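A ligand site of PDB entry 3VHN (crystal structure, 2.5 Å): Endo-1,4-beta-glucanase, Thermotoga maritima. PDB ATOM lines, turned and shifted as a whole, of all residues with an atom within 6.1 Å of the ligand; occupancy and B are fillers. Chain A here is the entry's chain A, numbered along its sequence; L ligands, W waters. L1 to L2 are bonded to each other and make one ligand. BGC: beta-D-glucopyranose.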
ATOM      1  N   GLU A  30     -20.198  14.370   6.836  1.00  0.00           N
ATOM      2  CA  GLU A  30     -20.145  13.222   5.961  1.00  0.00           C
ATOM      3  C   GLU A  30     -19.313  12.069   6.575  1.00  0.00           C
ATOM      4  O   GLU A  30     -18.171  12.251   7.001  1.00  0.00           O
ATOM      5  CB  GLU A  30     -19.526  13.595   4.622  1.00  0.00           C
ATOM      6  CG  GLU A  30     -19.796  12.492   3.634  1.00  0.00           C
ATOM      7  CD  GLU A  30     -19.174  12.672   2.246  1.00  0.00           C
ATOM      8  OE1 GLU A  30     -19.082  13.808   1.713  1.00  0.00           O
ATOM      9  OE2 GLU A  30     -18.809  11.639   1.654  1.00  0.00           O
ATOM     10  N   ASN A  32     -17.512   9.919   5.343  1.00  0.00           N
ATOM     11  CA  ASN A  32     -16.863   9.740   4.068  1.00  0.00           C
ATOM     12  C   ASN A  32     -15.829   8.621   3.952  1.00  0.00           C
ATOM     13  O   ASN A  32     -14.725   8.709   4.492  1.00  0.00           O
ATOM     14  CB  ASN A  32     -16.247  11.100   3.710  1.00  0.00           C
ATOM     15  CG  ASN A  32     -15.635  11.149   2.310  1.00  0.00           C
ATOM     16  OD1 ASN A  32     -15.742  10.231   1.502  1.00  0.00           O
ATOM     17  ND2 ASN A  32     -14.979  12.237   2.031  1.00  0.00           N
ATOM     18  N   TRP A  34     -14.889   7.455   0.901  1.00  0.00           N
ATOM     19  CA  TRP A  34     -14.889   7.398  -0.552  1.00  0.00           C
ATOM     20  C   TRP A  34     -14.035   6.396  -1.293  1.00  0.00           C
ATOM     21  O   TRP A  34     -14.441   5.882  -2.319  1.00  0.00           O
ATOM     22  CB  TRP A  34     -14.644   8.782  -1.115  1.00  0.00           C
ATOM     23  CG  TRP A  34     -13.299   9.223  -0.895  1.00  0.00           C
ATOM     24  CD1 TRP A  34     -12.810   9.924   0.188  1.00  0.00           C
ATOM     25  CD2 TRP A  34     -12.238   9.087  -1.809  1.00  0.00           C
ATOM     26  NE1 TRP A  34     -11.493  10.246  -0.010  1.00  0.00           N
ATOM     27  CE2 TRP A  34     -11.111   9.742  -1.232  1.00  0.00           C
ATOM     28  CE3 TRP A  34     -12.117   8.475  -3.055  1.00  0.00           C
ATOM     29  CZ2 TRP A  34      -9.880   9.815  -1.885  1.00  0.00           C
ATOM     30  CZ3 TRP A  34     -10.890   8.541  -3.696  1.00  0.00           C
ATOM     31  CH2 TRP A  34      -9.792   9.206  -3.107  1.00  0.00           C
ATOM     32  N   ARG A  68      -4.986   6.122  -5.490  1.00  0.00           N
ATOM     33  CA  ARG A  68      -5.335   7.379  -4.786  1.00  0.00           C
ATOM     34  C   ARG A  68      -4.710   7.429  -3.393  1.00  0.00           C
ATOM     35  O   ARG A  68      -4.759   8.475  -2.686  1.00  0.00           O
ATOM     36  CB  ARG A  68      -6.860   7.527  -4.643  1.00  0.00           C
ATOM     37  CG  ARG A  68      -7.630   7.642  -5.940  1.00  0.00           C
ATOM     38  CD  ARG A  68      -6.983   8.624  -6.888  1.00  0.00           C
ATOM     39  NE  ARG A  68      -6.857   9.966  -6.302  1.00  0.00           N
ATOM     40  CZ  ARG A  68      -7.868  10.800  -6.079  1.00  0.00           C
ATOM     41  NH1 ARG A  68      -9.113  10.450  -6.385  1.00  0.00           N
ATOM     42  NH2 ARG A  68      -7.610  12.000  -5.565  1.00  0.00           N
ATOM     43  N   VAL A  70      -5.076   7.244  -0.063  1.00  0.00           N
ATOM     44  CA  VAL A  70      -5.916   7.135   1.118  1.00  0.00           C
ATOM     45  C   VAL A  70      -7.184   6.356   0.921  1.00  0.00           C
ATOM     46  O   VAL A  70      -7.580   6.073  -0.229  1.00  0.00           O
ATOM     47  CB  VAL A  70      -6.265   8.483   1.704  1.00  0.00           C
ATOM     48  CG1 VAL A  70      -4.990   9.224   2.007  1.00  0.00           C
ATOM     49  CG2 VAL A  70      -7.185   9.266   0.763  1.00  0.00           C
ATOM     50  N   GLY A  72     -10.212   7.033   3.125  1.00  0.00           N
ATOM     51  CA  GLY A  72     -11.405   7.728   3.499  1.00  0.00           C
ATOM     52  C   GLY A  72     -11.111   9.040   4.173  1.00  0.00           C
ATOM     53  O   GLY A  72      -9.935   9.339   4.465  1.00  0.00           O
ATOM     54  N   TYR A  73     -12.171   9.812   4.416  1.00  0.00           N
ATOM     55  CA  TYR A  73     -12.048  11.137   4.992  1.00  0.00           C
ATOM     56  C   TYR A  73     -13.283  11.620   5.773  1.00  0.00           C
ATOM     57  O   TYR A  73     -13.921  12.586   5.373  1.00  0.00           O
ATOM     58  CB  TYR A  73     -11.734  12.136   3.863  1.00  0.00           C
ATOM     59  CG  TYR A  73     -11.490  13.581   4.275  1.00  0.00           C
ATOM     60  CD1 TYR A  73     -10.548  13.909   5.234  1.00  0.00           C
ATOM     61  CD2 TYR A  73     -12.167  14.629   3.640  1.00  0.00           C
ATOM     62  CE1 TYR A  73     -10.254  15.214   5.574  1.00  0.00           C
ATOM     63  CE2 TYR A  73     -11.902  15.974   3.957  1.00  0.00           C
ATOM     64  CZ  TYR A  73     -10.931  16.262   4.939  1.00  0.00           C
ATOM     65  OH  TYR A  73     -10.633  17.583   5.288  1.00  0.00           O
ATOM     66  N   GLU A  75     -15.636  13.634   7.908  1.00  0.00           N
ATOM     67  CA  GLU A  75     -15.440  15.090   8.029  1.00  0.00           C
ATOM     68  C   GLU A  75     -16.771  15.815   8.226  1.00  0.00           C
ATOM     69  O   GLU A  75     -17.826  15.191   8.228  1.00  0.00           O
ATOM     70  CB  GLU A  75     -14.912  15.535   6.690  1.00  0.00           C
ATOM     71  CG  GLU A  75     -15.918  15.083   5.579  1.00  0.00           C
ATOM     72  CD  GLU A  75     -15.706  15.735   4.188  1.00  0.00           C
ATOM     73  OE1 GLU A  75     -15.496  16.988   4.110  1.00  0.00           O
ATOM     74  OE2 GLU A  75     -15.765  15.002   3.144  1.00  0.00           O
ATOM     75  N   LYS A  81     -19.909  21.295  -1.225  1.00  0.00           N
ATOM     76  CA  LYS A  81     -18.881  20.336  -1.682  1.00  0.00           C
ATOM     77  C   LYS A  81     -19.225  19.903  -3.133  1.00  0.00           C
ATOM     78  O   LYS A  81     -20.147  19.138  -3.369  1.00  0.00           O
ATOM     79  CB  LYS A  81     -18.859  19.132  -0.733  1.00  0.00           C
ATOM     80  CG  LYS A  81     -17.765  18.135  -1.040  1.00  0.00           C
ATOM     81  CD  LYS A  81     -17.706  17.044  -0.013  1.00  0.00           C
ATOM     82  CE  LYS A  81     -16.892  15.889  -0.557  1.00  0.00           C
ATOM     83  NZ  LYS A  81     -16.269  15.053   0.476  1.00  0.00           N
ATOM     84  N   TRP A  83     -18.197  17.687  -5.259  1.00  0.00           N
ATOM     85  CA  TRP A  83     -18.361  16.250  -5.484  1.00  0.00           C
ATOM     86  C   TRP A  83     -19.694  15.610  -5.050  1.00  0.00           C
ATOM     87  O   TRP A  83     -20.133  14.573  -5.595  1.00  0.00           O
ATOM     88  CB  TRP A  83     -17.202  15.529  -4.824  1.00  0.00           C
ATOM     89  CG  TRP A  83     -15.852  15.872  -5.414  1.00  0.00           C
ATOM     90  CD1 TRP A  83     -14.883  16.677  -4.853  1.00  0.00           C
ATOM     91  CD2 TRP A  83     -15.319  15.409  -6.667  1.00  0.00           C
ATOM     92  NE1 TRP A  83     -13.781  16.730  -5.681  1.00  0.00           N
ATOM     93  CE2 TRP A  83     -14.022  15.961  -6.794  1.00  0.00           C
ATOM     94  CE3 TRP A  83     -15.825  14.573  -7.692  1.00  0.00           C
ATOM     95  CZ2 TRP A  83     -13.214  15.711  -7.906  1.00  0.00           C
ATOM     96  CZ3 TRP A  83     -15.017  14.323  -8.804  1.00  0.00           C
ATOM     97  CH2 TRP A  83     -13.720  14.895  -8.904  1.00  0.00           C
ATOM     98  N   GLU A  84     -20.360  16.231  -4.098  1.00  0.00           N
ATOM     99  CA  GLU A  84     -21.614  15.672  -3.605  1.00  0.00           C
ATOM    100  C   GLU A  84     -22.769  16.536  -4.049  1.00  0.00           C
ATOM    101  O   GLU A  84     -23.936  16.214  -3.853  1.00  0.00           O
ATOM    102  CB  GLU A  84     -21.599  15.552  -2.089  1.00  0.00           C
ATOM    103  CG  GLU A  84     -20.612  14.505  -1.562  1.00  0.00           C
ATOM    104  CD  GLU A  84     -20.924  13.088  -2.047  1.00  0.00           C
ATOM    105  OE1 GLU A  84     -22.130  12.759  -2.257  1.00  0.00           O
ATOM    106  OE2 GLU A  84     -19.969  12.311  -2.210  1.00  0.00           O
ATOM    107  N   GLU A 124      -9.610  21.440   4.019  1.00  0.00           N
ATOM    108  CA  GLU A 124      -9.414  21.797   2.619  1.00  0.00           C
ATOM    109  C   GLU A 124     -10.595  22.489   1.954  1.00  0.00           C
ATOM    110  O   GLU A 124     -11.737  22.460   2.425  1.00  0.00           O
ATOM    111  CB  GLU A 124      -9.073  20.539   1.796  1.00  0.00           C
ATOM    112  CG  GLU A 124     -10.276  19.647   1.536  1.00  0.00           C
ATOM    113  CD  GLU A 124     -10.028  18.605   0.439  1.00  0.00           C
ATOM    114  OE1 GLU A 124     -10.820  17.658   0.325  1.00  0.00           O
ATOM    115  OE2 GLU A 124      -9.062  18.724  -0.324  1.00  0.00           O
ATOM    116  N   TRP A 126     -12.140  23.451  -2.232  1.00  0.00           N
ATOM    117  CA  TRP A 126     -12.086  23.169  -3.652  1.00  0.00           C
ATOM    118  C   TRP A 126     -12.393  24.457  -4.383  1.00  0.00           C
ATOM    119  O   TRP A 126     -13.474  25.002  -4.224  1.00  0.00           O
ATOM    120  CB  TRP A 126     -13.131  22.158  -4.013  1.00  0.00           C
ATOM    121  CG  TRP A 126     -12.873  20.840  -3.421  1.00  0.00           C
ATOM    122  CD1 TRP A 126     -13.355  20.361  -2.217  1.00  0.00           C
ATOM    123  CD2 TRP A 126     -12.105  19.802  -3.993  1.00  0.00           C
ATOM    124  NE1 TRP A 126     -12.938  19.077  -2.036  1.00  0.00           N
ATOM    125  CE2 TRP A 126     -12.165  18.701  -3.101  1.00  0.00           C
ATOM    126  CE3 TRP A 126     -11.369  19.676  -5.181  1.00  0.00           C
ATOM    127  CZ2 TRP A 126     -11.526  17.490  -3.374  1.00  0.00           C
ATOM    128  CZ3 TRP A 126     -10.729  18.474  -5.449  1.00  0.00           C
ATOM    129  CH2 TRP A 126     -10.820  17.393  -4.564  1.00  0.00           C
ATOM    130  N   GLU A 142      -7.468  21.974  -5.589  1.00  0.00           N
ATOM    131  CA  GLU A 142      -7.816  21.380  -4.303  1.00  0.00           C
ATOM    132  C   GLU A 142      -6.689  21.922  -3.405  1.00  0.00           C
ATOM    133  O   GLU A 142      -5.503  21.826  -3.770  1.00  0.00           O
ATOM    134  CB  GLU A 142      -7.759  19.848  -4.341  1.00  0.00           C
ATOM    135  CG  GLU A 142      -7.917  19.182  -2.940  1.00  0.00           C
ATOM    136  CD  GLU A 142      -7.809  17.630  -2.955  1.00  0.00           C
ATOM    137  OE1 GLU A 142      -7.347  17.065  -3.969  1.00  0.00           O
ATOM    138  OE2 GLU A 142      -8.167  16.987  -1.929  1.00  0.00           O
ATOM    139  N   MET A 144      -5.309  21.831   0.623  1.00  0.00           N
ATOM    140  CA  MET A 144      -5.428  21.306   1.969  1.00  0.00           C
ATOM    141  C   MET A 144      -4.474  21.942   2.894  1.00  0.00           C
ATOM    142  O   MET A 144      -3.426  22.456   2.494  1.00  0.00           O
ATOM    143  CB  MET A 144      -5.151  19.844   2.013  1.00  0.00           C
ATOM    144  CG  MET A 144      -5.615  19.088   0.836  1.00  0.00           C
ATOM    145  SD  MET A 144      -5.628  17.342   1.195  1.00  0.00           S
ATOM    146  CE  MET A 144      -7.194  17.145   1.999  1.00  0.00           C
ATOM    147  N   TRP A 184      -2.594  16.525 -11.103  1.00  0.00           N
ATOM    148  CA  TRP A 184      -3.293  15.357 -11.592  1.00  0.00           C
ATOM    149  C   TRP A 184      -4.507  15.804 -12.429  1.00  0.00           C
ATOM    150  O   TRP A 184      -4.393  16.610 -13.349  1.00  0.00           O
ATOM    151  CB  TRP A 184      -3.806  14.539 -10.417  1.00  0.00           C
ATOM    152  CG  TRP A 184      -2.775  14.114  -9.404  1.00  0.00           C
ATOM    153  CD1 TRP A 184      -1.533  13.550  -9.655  1.00  0.00           C
ATOM    154  CD2 TRP A 184      -2.961  14.067  -7.982  1.00  0.00           C
ATOM    155  NE1 TRP A 184      -0.951  13.153  -8.465  1.00  0.00           N
ATOM    156  CE2 TRP A 184      -1.802  13.448  -7.418  1.00  0.00           C
ATOM    157  CE3 TRP A 184      -4.000  14.481  -7.115  1.00  0.00           C
ATOM    158  CZ2 TRP A 184      -1.660  13.232  -6.035  1.00  0.00           C
ATOM    159  CZ3 TRP A 184      -3.860  14.257  -5.737  1.00  0.00           C
ATOM    160  CH2 TRP A 184      -2.691  13.639  -5.219  1.00  0.00           C
ATOM    161  N   TRP A 186      -6.601  17.648 -11.416  1.00  0.00           N
ATOM    162  CA  TRP A 186      -6.768  19.035 -10.992  1.00  0.00           C
ATOM    163  C   TRP A 186      -5.488  19.417 -10.260  1.00  0.00           C
ATOM    164  O   TRP A 186      -4.591  18.604 -10.080  1.00  0.00           O
ATOM    165  CB  TRP A 186      -7.973  19.216 -10.076  1.00  0.00           C
ATOM    166  CG  TRP A 186      -8.019  18.287  -8.857  1.00  0.00           C
ATOM    167  CD1 TRP A 186      -7.430  18.506  -7.628  1.00  0.00           C
ATOM    168  CD2 TRP A 186      -8.688  17.024  -8.757  1.00  0.00           C
ATOM    169  NE1 TRP A 186      -7.719  17.465  -6.778  1.00  0.00           N
ATOM    170  CE2 TRP A 186      -8.486  16.538  -7.446  1.00  0.00           C
ATOM    171  CE3 TRP A 186      -9.431  16.255  -9.649  1.00  0.00           C
ATOM    172  CZ2 TRP A 186      -9.015  15.320  -6.995  1.00  0.00           C
ATOM    173  CZ3 TRP A 186      -9.971  15.019  -9.204  1.00  0.00           C
ATOM    174  CH2 TRP A 186      -9.758  14.582  -7.880  1.00  0.00           C
ATOM    175  N   TYR A 188      -3.384  20.109  -7.118  1.00  0.00           N
ATOM    176  CA  TYR A 188      -3.404  19.725  -5.742  1.00  0.00           C
ATOM    177  C   TYR A 188      -2.310  20.403  -4.950  1.00  0.00           C
ATOM    178  O   TYR A 188      -1.136  20.268  -5.264  1.00  0.00           O
ATOM    179  CB  TYR A 188      -3.244  18.220  -5.650  1.00  0.00           C
ATOM    180  CG  TYR A 188      -2.958  17.678  -4.266  1.00  0.00           C
ATOM    181  CD1 TYR A 188      -3.968  17.182  -3.439  1.00  0.00           C
ATOM    182  CD2 TYR A 188      -1.646  17.639  -3.783  1.00  0.00           C
ATOM    183  CE1 TYR A 188      -3.688  16.638  -2.190  1.00  0.00           C
ATOM    184  CE2 TYR A 188      -1.336  17.105  -2.562  1.00  0.00           C
ATOM    185  CZ  TYR A 188      -2.355  16.607  -1.771  1.00  0.00           C
ATOM    186  OH  TYR A 188      -1.975  15.964  -0.641  1.00  0.00           O
ATOM    187  N   GLU A 235     -13.820  22.159   4.433  1.00  0.00           N
ATOM    188  CA  GLU A 235     -13.993  20.833   5.016  1.00  0.00           C
ATOM    189  C   GLU A 235     -13.014  20.630   6.144  1.00  0.00           C
ATOM    190  O   GLU A 235     -11.893  21.099   6.091  1.00  0.00           O
ATOM    191  CB  GLU A 235     -13.805  19.732   3.960  1.00  0.00           C
ATOM    192  CG  GLU A 235     -14.676  19.938   2.736  1.00  0.00           C
ATOM    193  CD  GLU A 235     -14.519  18.907   1.625  1.00  0.00           C
ATOM    194  OE1 GLU A 235     -14.914  17.729   1.807  1.00  0.00           O
ATOM    195  OE2 GLU A 235     -14.029  19.268   0.527  1.00  0.00           O
ATOM    196  N   GLU A 239      -8.004  12.195   7.116  1.00  0.00           N
ATOM    197  CA  GLU A 239      -7.856  11.174   6.072  1.00  0.00           C
ATOM    198  C   GLU A 239      -7.156  10.004   6.692  1.00  0.00           C
ATOM    199  O   GLU A 239      -6.307  10.174   7.607  1.00  0.00           O
ATOM    200  CB  GLU A 239      -6.947  11.625   4.924  1.00  0.00           C
ATOM    201  CG  GLU A 239      -7.291  12.949   4.324  1.00  0.00           C
ATOM    202  CD  GLU A 239      -6.526  13.125   3.046  1.00  0.00           C
ATOM    203  OE1 GLU A 239      -5.546  13.914   3.081  1.00  0.00           O
ATOM    204  OE2 GLU A 239      -6.911  12.448   2.034  1.00  0.00           O
HETATM  205  C2  BGC L   1      -7.767  13.707  -2.886  1.00  0.00           C
HETATM  206  C3  BGC L   1      -9.267  13.972  -2.998  1.00  0.00           C
HETATM  207  C4  BGC L   1      -9.994  13.608  -1.705  1.00  0.00           C
HETATM  208  C5  BGC L   1      -9.294  14.257  -0.508  1.00  0.00           C
HETATM  209  C6  BGC L   1      -9.950  13.921   0.838  1.00  0.00           C
HETATM  210  C1  BGC L   1      -7.199  14.296  -1.588  1.00  0.00           C
HETATM  211  O1  BGC L   1      -5.867  13.828  -1.421  1.00  0.00           O
HETATM  212  O2  BGC L   1      -7.133  14.353  -3.996  1.00  0.00           O
HETATM  213  O3  BGC L   1      -9.770  13.184  -4.088  1.00  0.00           O
HETATM  214  O4  BGC L   1     -11.321  14.160  -1.778  1.00  0.00           O
HETATM  215  O5  BGC L   1      -7.936  13.813  -0.452  1.00  0.00           O
HETATM  216  O6  BGC L   1      -9.751  12.544   1.183  1.00  0.00           O
HETATM  217  C2  BGC L   2     -13.647  13.702  -1.817  1.00  0.00           C
HETATM  218  C3  BGC L   2     -14.720  12.740  -2.319  1.00  0.00           C
HETATM  219  C4  BGC L   2     -14.620  12.673  -3.844  1.00  0.00           C
HETATM  220  C5  BGC L   2     -13.201  12.274  -4.250  1.00  0.00           C
HETATM  221  C6  BGC L   2     -13.139  12.236  -5.773  1.00  0.00           C
HETATM  222  C1  BGC L   2     -12.279  13.213  -2.277  1.00  0.00           C
HETATM  223  O2  BGC L   2     -13.714  13.745  -0.384  1.00  0.00           O
HETATM  224  O3  BGC L   2     -16.005  13.185  -1.887  1.00  0.00           O
HETATM  225  O4  BGC L   2     -15.518  11.666  -4.314  1.00  0.00           O
HETATM  226  O5  BGC L   2     -12.241  13.199  -3.713  1.00  0.00           O
HETATM  227  O6  BGC L   2     -11.851  11.757  -6.188  1.00  0.00           O
HETATM  228  O   HOH W   1     -18.159  11.757  -4.599  1.00  0.00           O
HETATM  229  O   HOH W   2      -5.370  11.426  -2.745  1.00  0.00           O
HETATM  230  O   HOH W   3     -12.751   9.139  -6.888  1.00  0.00           O
HETATM  231  O   HOH W   4     -17.821  11.452  -0.825  1.00  0.00           O
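Residues that only touch the ligand: Tyr 73 (3.4 Å), Tyr 188 (3.6 Å), Trp 186 (3.7 Å), Trp 126 (3.7 Å), Trp 184 (3.7 Å), Trp 83 (3.8 Å) and Glu 124 (3.8 Å).
Hydrophobic or aromatic side chains within 4 Å of the ligand: Trp 34, Tyr 73, Trp 83, Trp 126, Trp 184, Trp 186 and Tyr 188.
Of the 20 residues printed, 13 come within 4 Å of the ligand.
The nearest printed residue that does not touch the ligand is Glu 84 (4.1 Å).
NZ of Lys 81 sits at hydrogen-bond distance from O2 of BGC L2 (3.0 Å).
The side-chain amide nitrogen (ND2) of Asn 32 is in hydrogen-bond range of an oxygen (O2) of BGC L2.
O2 of BGC L1 is in hydrogen-bond range of NH2 of Arg 68 (2.9 Å).
The side-chain carboxylate of Glu 142 lies within hydrogen-bond range of an oxygen (O2) of BGC L1.
NE1 of Trp 34 lies within hydrogen-bond range of O6 of BGC L1, 3.1 Å away.
O6 of BGC L1 is in hydrogen-bond range of OE2 of Glu 239, at 3.0 Å.
Water W1 bridges an oxygen (O4) of BGC L2 and the side-chain carboxylate (OE2) of Glu 84.
Water W2 lies within hydrogen-bond range of an oxygen (O1) of BGC L1 (2.8 Å) and the backbone carbonyl oxygen of Arg 68 (3.0 Å).
The side-chain amino group (NZ) of Lys 81 lies within salt-bridge range of the side-chain carboxylate (OE1) of Glu 30.
N of Glu 235 sits at hydrogen-bond distance from O of Glu 124.
OE2 of Glu 75 is in salt-bridge range of NZ of Lys 81 (2.7 Å).
The side-chain carboxylate (OE1) of Glu 235 lies within salt-bridge range of the side-chain amino group (NZ) of Lys 81 (3.3 Å).
OE2 of Glu 124 sits close to OE2 of Glu 142.
OE1 of Glu 124 sits at hydrogen-bond distance from NE1 of Trp 126, 3.5 Å away.
The side-chain amide nitrogen of Asn 32 sits at hydrogen-bond distance from the side-chain carboxylate of Glu 75 (3.1 Å).
The side-chain amino group (NZ) of Lys 81 lies close to the side-chain amide nitrogen (ND2) of Asn 32, at 3.5 Å.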
